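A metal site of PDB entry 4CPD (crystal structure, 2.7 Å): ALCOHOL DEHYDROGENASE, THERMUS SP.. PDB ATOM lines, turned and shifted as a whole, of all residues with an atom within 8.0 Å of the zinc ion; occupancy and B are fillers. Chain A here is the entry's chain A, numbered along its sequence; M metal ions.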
ATOM      1  N   ILE A  87     -17.868  -4.816  -2.781  1.00  0.00           N
ATOM      2  CA  ILE A  87     -18.584  -5.688  -1.880  1.00  0.00           C
ATOM      3  C   ILE A  87     -17.636  -6.525  -1.099  1.00  0.00           C
ATOM      4  O   ILE A  87     -16.498  -6.723  -1.501  1.00  0.00           O
ATOM      5  CB  ILE A  87     -19.592  -6.594  -2.622  1.00  0.00           C
ATOM      6  CG1 ILE A  87     -18.886  -7.586  -3.546  1.00  0.00           C
ATOM      7  CG2 ILE A  87     -20.538  -5.761  -3.465  1.00  0.00           C
ATOM      8  CD1 ILE A  87     -19.709  -8.837  -3.835  1.00  0.00           C
ATOM      9  N   ALA A  88     -18.128  -7.049   0.015  1.00  0.00           N
ATOM     10  CA  ALA A  88     -17.334  -7.733   0.996  1.00  0.00           C
ATOM     11  C   ALA A  88     -18.220  -8.711   1.729  1.00  0.00           C
ATOM     12  O   ALA A  88     -19.403  -8.463   1.881  1.00  0.00           O
ATOM     13  CB  ALA A  88     -16.699  -6.758   1.964  1.00  0.00           C
ATOM     14  N   CYS A  89     -17.625  -9.800   2.195  1.00  0.00           N
ATOM     15  CA  CYS A  89     -18.375 -10.937   2.659  1.00  0.00           C
ATOM     16  C   CYS A  89     -18.528 -10.891   4.168  1.00  0.00           C
ATOM     17  O   CYS A  89     -19.476 -11.455   4.696  1.00  0.00           O
ATOM     18  CB  CYS A  89     -17.654 -12.240   2.237  1.00  0.00           C
ATOM     19  SG  CYS A  89     -16.212 -12.714   3.250  1.00  0.00           S
ATOM     20  N   GLY A  90     -17.540 -10.337   4.850  1.00  0.00           N
ATOM     21  CA  GLY A  90     -17.593 -10.182   6.282  1.00  0.00           C
ATOM     22  C   GLY A  90     -17.037 -11.342   7.102  1.00  0.00           C
ATOM     23  O   GLY A  90     -16.978 -11.261   8.352  1.00  0.00           O
ATOM     24  N   THR A  91     -16.655 -12.437   6.452  1.00  0.00           N
ATOM     25  CA  THR A  91     -16.179 -13.618   7.182  1.00  0.00           C
ATOM     26  C   THR A  91     -14.824 -14.164   6.730  1.00  0.00           C
ATOM     27  O   THR A  91     -14.187 -14.895   7.470  1.00  0.00           O
ATOM     28  CB  THR A  91     -17.245 -14.770   7.229  1.00  0.00           C
ATOM     29  OG1 THR A  91     -17.645 -15.132   5.897  1.00  0.00           O
ATOM     30  CG2 THR A  91     -18.472 -14.358   8.055  1.00  0.00           C
ATOM     31  N   CYS A  92     -14.346 -13.809   5.540  1.00  0.00           N
ATOM     32  CA  CYS A  92     -13.011 -14.239   5.143  1.00  0.00           C
ATOM     33  C   CYS A  92     -11.930 -13.572   6.004  1.00  0.00           C
ATOM     34  O   CYS A  92     -12.172 -12.578   6.699  1.00  0.00           O
ATOM     35  CB  CYS A  92     -12.777 -13.929   3.695  1.00  0.00           C
ATOM     36  SG  CYS A  92     -12.462 -12.228   3.301  1.00  0.00           S
ATOM     37  N   PRO A  93     -10.706 -14.139   5.970  1.00  0.00           N
ATOM     38  CA  PRO A  93      -9.645 -13.587   6.820  1.00  0.00           C
ATOM     39  C   PRO A  93      -9.365 -12.095   6.628  1.00  0.00           C
ATOM     40  O   PRO A  93      -9.109 -11.391   7.633  1.00  0.00           O
ATOM     41  CB  PRO A  93      -8.420 -14.409   6.412  1.00  0.00           C
ATOM     42  CG  PRO A  93      -8.973 -15.664   5.816  1.00  0.00           C
ATOM     43  CD  PRO A  93     -10.209 -15.230   5.127  1.00  0.00           C
ATOM     44  N   TYR A  94      -9.428 -11.621   5.380  1.00  0.00           N
ATOM     45  CA  TYR A  94      -9.298 -10.177   5.121  1.00  0.00           C
ATOM     46  C   TYR A  94     -10.431  -9.312   5.740  1.00  0.00           C
ATOM     47  O   TYR A  94     -10.167  -8.268   6.311  1.00  0.00           O
ATOM     48  CB  TYR A  94      -9.098  -9.895   3.622  1.00  0.00           C
ATOM     49  CG  TYR A  94      -7.750 -10.399   3.178  1.00  0.00           C
ATOM     50  CD1 TYR A  94      -6.595  -9.692   3.488  1.00  0.00           C
ATOM     51  CD2 TYR A  94      -7.609 -11.653   2.543  1.00  0.00           C
ATOM     52  CE1 TYR A  94      -5.339 -10.184   3.133  1.00  0.00           C
ATOM     53  CE2 TYR A  94      -6.369 -12.140   2.177  1.00  0.00           C
ATOM     54  CZ  TYR A  94      -5.230 -11.411   2.464  1.00  0.00           C
ATOM     55  OH  TYR A  94      -3.978 -11.892   2.100  1.00  0.00           O
ATOM     56  N   CYS A  95     -11.672  -9.773   5.651  1.00  0.00           N
ATOM     57  CA  CYS A  95     -12.778  -9.065   6.246  1.00  0.00           C
ATOM     58  C   CYS A  95     -12.609  -9.047   7.736  1.00  0.00           C
ATOM     59  O   CYS A  95     -12.885  -8.038   8.339  1.00  0.00           O
ATOM     60  CB  CYS A  95     -14.144  -9.692   5.897  1.00  0.00           C
ATOM     61  SG  CYS A  95     -14.694  -9.334   4.214  1.00  0.00           S
ATOM     62  N   ARG A  96     -12.129 -10.133   8.326  1.00  0.00           N
ATOM     63  CA  ARG A  96     -11.938 -10.170   9.798  1.00  0.00           C
ATOM     64  C   ARG A  96     -10.840  -9.199  10.293  1.00  0.00           C
ATOM     65  O   ARG A  96     -10.900  -8.747  11.429  1.00  0.00           O
ATOM     66  CB  ARG A  96     -11.666 -11.575  10.293  1.00  0.00           C
ATOM     67  CG  ARG A  96     -12.620 -12.597   9.707  1.00  0.00           C
ATOM     68  CD  ARG A  96     -13.168 -13.564  10.728  1.00  0.00           C
ATOM     69  NE  ARG A  96     -14.513 -13.178  11.125  1.00  0.00           N
ATOM     70  CZ  ARG A  96     -15.603 -13.942  11.067  1.00  0.00           C
ATOM     71  NH1 ARG A  96     -15.563 -15.217  10.657  1.00  0.00           N
ATOM     72  NH2 ARG A  96     -16.764 -13.445  11.465  1.00  0.00           N
ATOM     73  N   GLN A  99     -10.069  -5.337   6.492  1.00  0.00           N
ATOM     74  CA  GLN A  99      -9.567  -4.920   5.194  1.00  0.00           C
ATOM     75  C   GLN A  99     -10.521  -5.425   4.103  1.00  0.00           C
ATOM     76  O   GLN A  99     -10.231  -6.336   3.324  1.00  0.00           O
ATOM     77  CB  GLN A  99      -8.153  -5.450   4.994  1.00  0.00           C
ATOM     78  CG  GLN A  99      -7.184  -4.985   6.066  1.00  0.00           C
ATOM     79  CD  GLN A  99      -5.766  -5.455   5.788  1.00  0.00           C
ATOM     80  OE1 GLN A  99      -5.526  -6.647   5.642  1.00  0.00           O
ATOM     81  NE2 GLN A  99      -4.825  -4.516   5.707  1.00  0.00           N
ATOM     82  N   TYR A 100     -11.689  -4.795   4.071  1.00  0.00           N
ATOM     83  CA  TYR A 100     -12.823  -5.264   3.271  1.00  0.00           C
ATOM     84  C   TYR A 100     -12.545  -5.095   1.797  1.00  0.00           C
ATOM     85  O   TYR A 100     -13.123  -5.799   0.973  1.00  0.00           O
ATOM     86  CB  TYR A 100     -14.130  -4.538   3.639  1.00  0.00           C
ATOM     87  CG  TYR A 100     -14.448  -4.556   5.135  1.00  0.00           C
ATOM     88  CD1 TYR A 100     -15.176  -5.595   5.714  1.00  0.00           C
ATOM     89  CD2 TYR A 100     -13.982  -3.532   5.988  1.00  0.00           C
ATOM     90  CE1 TYR A 100     -15.444  -5.612   7.077  1.00  0.00           C
ATOM     91  CE2 TYR A 100     -14.259  -3.546   7.346  1.00  0.00           C
ATOM     92  CZ  TYR A 100     -15.000  -4.595   7.885  1.00  0.00           C
ATOM     93  OH  TYR A 100     -15.244  -4.607   9.232  1.00  0.00           O
ATOM     94  N   ASN A 101     -11.680  -4.165   1.437  1.00  0.00           N
ATOM     95  CA  ASN A 101     -11.251  -4.064   0.043  1.00  0.00           C
ATOM     96  C   ASN A 101     -10.410  -5.253  -0.449  1.00  0.00           C
ATOM     97  O   ASN A 101     -10.178  -5.363  -1.615  1.00  0.00           O
ATOM     98  CB  ASN A 101     -10.442  -2.782  -0.178  1.00  0.00           C
ATOM     99  CG  ASN A 101      -9.238  -2.684   0.736  1.00  0.00           C
ATOM    100  OD1 ASN A 101      -9.341  -2.928   1.931  1.00  0.00           O
ATOM    101  ND2 ASN A 101      -8.094  -2.381   0.168  1.00  0.00           N
ATOM    102  N   LEU A 102      -9.908  -6.097   0.457  1.00  0.00           N
ATOM    103  CA  LEU A 102      -9.188  -7.295   0.055  1.00  0.00           C
ATOM    104  C   LEU A 102      -9.993  -8.558   0.240  1.00  0.00           C
ATOM    105  O   LEU A 102      -9.408  -9.656   0.251  1.00  0.00           O
ATOM    106  CB  LEU A 102      -7.898  -7.396   0.859  1.00  0.00           C
ATOM    107  CG  LEU A 102      -6.985  -6.178   0.641  1.00  0.00           C
ATOM    108  CD1 LEU A 102      -5.782  -6.272   1.580  1.00  0.00           C
ATOM    109  CD2 LEU A 102      -6.553  -6.080  -0.815  1.00  0.00           C
ATOM    110  N   CYS A 103     -11.317  -8.413   0.405  1.00  0.00           N
ATOM    111  CA  CYS A 103     -12.231  -9.540   0.639  1.00  0.00           C
ATOM    112  C   CYS A 103     -12.000 -10.594  -0.438  1.00  0.00           C
ATOM    113  O   CYS A 103     -11.857 -10.263  -1.606  1.00  0.00           O
ATOM    114  CB  CYS A 103     -13.678  -9.105   0.574  1.00  0.00           C
ATOM    115  SG  CYS A 103     -14.786 -10.508   0.744  1.00  0.00           S
ATOM    116  N   GLU A 104     -11.941 -11.846  -0.008  1.00  0.00           N
ATOM    117  CA  GLU A 104     -11.688 -12.969  -0.936  1.00  0.00           C
ATOM    118  C   GLU A 104     -12.849 -13.236  -1.884  1.00  0.00           C
ATOM    119  O   GLU A 104     -12.646 -13.698  -2.983  1.00  0.00           O
ATOM    120  CB  GLU A 104     -11.295 -14.234  -0.164  1.00  0.00           C
ATOM    121  CG  GLU A 104      -9.775 -14.415  -0.065  1.00  0.00           C
ATOM    122  CD  GLU A 104      -9.346 -15.215   1.139  1.00  0.00           C
ATOM    123  OE1 GLU A 104     -10.271 -15.765   1.786  1.00  0.00           O
ATOM    124  OE2 GLU A 104      -8.128 -15.286   1.445  1.00  0.00           O
ATOM    125  N   ARG A 105     -14.060 -12.916  -1.456  1.00  0.00           N
ATOM    126  CA  ARG A 105     -15.244 -12.905  -2.342  1.00  0.00           C
ATOM    127  C   ARG A 105     -15.564 -11.472  -2.828  1.00  0.00           C
ATOM    128  O   ARG A 105     -16.713 -11.140  -3.146  1.00  0.00           O
ATOM    129  CB  ARG A 105     -16.425 -13.498  -1.597  1.00  0.00           C
ATOM    130  CG  ARG A 105     -16.356 -15.009  -1.482  1.00  0.00           C
ATOM    131  CD  ARG A 105     -17.447 -15.557  -0.579  1.00  0.00           C
ATOM    132  NE  ARG A 105     -16.925 -15.502   0.772  1.00  0.00           N
ATOM    133  CZ  ARG A 105     -16.376 -16.509   1.434  1.00  0.00           C
ATOM    134  NH1 ARG A 105     -16.358 -17.739   0.905  1.00  0.00           N
ATOM    135  NH2 ARG A 105     -15.896 -16.272   2.654  1.00  0.00           N
ATOM    136  N   GLY A 106     -14.540 -10.639  -2.888  1.00  0.00           N
ATOM    137  CA  GLY A 106     -14.730  -9.235  -3.173  1.00  0.00           C
ATOM    138  C   GLY A 106     -15.094  -8.997  -4.605  1.00  0.00           C
ATOM    139  O   GLY A 106     -14.823  -9.838  -5.441  1.00  0.00           O
ATOM    140  N   PHE A 130     -24.804  -9.771   0.652  1.00  0.00           N
ATOM    141  CA  PHE A 130     -24.309  -9.522   2.002  1.00  0.00           C
ATOM    142  C   PHE A 130     -24.677  -8.086   2.454  1.00  0.00           C
ATOM    143  O   PHE A 130     -23.843  -7.324   2.961  1.00  0.00           O
ATOM    144  CB  PHE A 130     -22.769  -9.724   2.046  1.00  0.00           C
ATOM    145  CG  PHE A 130     -22.284 -11.089   1.590  1.00  0.00           C
ATOM    146  CD1 PHE A 130     -22.596 -12.246   2.308  1.00  0.00           C
ATOM    147  CD2 PHE A 130     -21.475 -11.192   0.454  1.00  0.00           C
ATOM    148  CE1 PHE A 130     -22.127 -13.480   1.886  1.00  0.00           C
ATOM    149  CE2 PHE A 130     -20.990 -12.425   0.026  1.00  0.00           C
ATOM    150  CZ  PHE A 130     -21.326 -13.567   0.749  1.00  0.00           C
ATOM    151  N   VAL A 133     -23.446  -6.361   5.396  1.00  0.00           N
ATOM    152  CA  VAL A 133     -22.125  -5.759   5.376  1.00  0.00           C
ATOM    153  C   VAL A 133     -22.074  -4.536   4.447  1.00  0.00           C
ATOM    154  O   VAL A 133     -21.409  -3.544   4.755  1.00  0.00           O
ATOM    155  CB  VAL A 133     -21.117  -6.796   4.851  1.00  0.00           C
ATOM    156  CG1 VAL A 133     -19.749  -6.193   4.607  1.00  0.00           C
ATOM    157  CG2 VAL A 133     -21.024  -7.969   5.818  1.00  0.00           C
HETATM  158 ZN    ZN M   1     -14.559 -11.169   2.797  1.00  0.00          ZN
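The side-chain sulfur (SG) of Cys 103 is bound to the zinc ion, at 2.2 Å.
The zinc ion is bound by SG of Cys 89, at 2.3 Å.
The side-chain sulfur (SG) of Cys 95 binds the zinc ion (2.3 Å).
SG of Cys 92 is bound to the zinc ion (2.4 Å).
SG of Cys 103 sits close to N of Arg 105 (3.3 Å).
The side-chain sulfur of Cys 103 sits close to the backbone NH of Gly 106, at 3.6 Å.
SG of Cys 89 lies close to N of Thr 91, 3.2 Å away.
The guanidinium group (NH2) of Arg 105 lies close to the side-chain sulfur (SG) of Cys 89 (3.6 Å).
N of Gly 90 sits close to SG of Cys 95.
SG of Cys 92 sits close to N of Glu 104.
SG of Cys 92 lies close to N of Tyr 94 (3.7 Å).
N of Gly 90 touches the zinc ion (3.7 Å).
N of Glu 104 touches the zinc ion, 3.9 Å away.
Within 4 Å of the zinc ion: Cys 89, Gly 90, Cys 92, Cys 95, Cys 103 and Glu 104.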
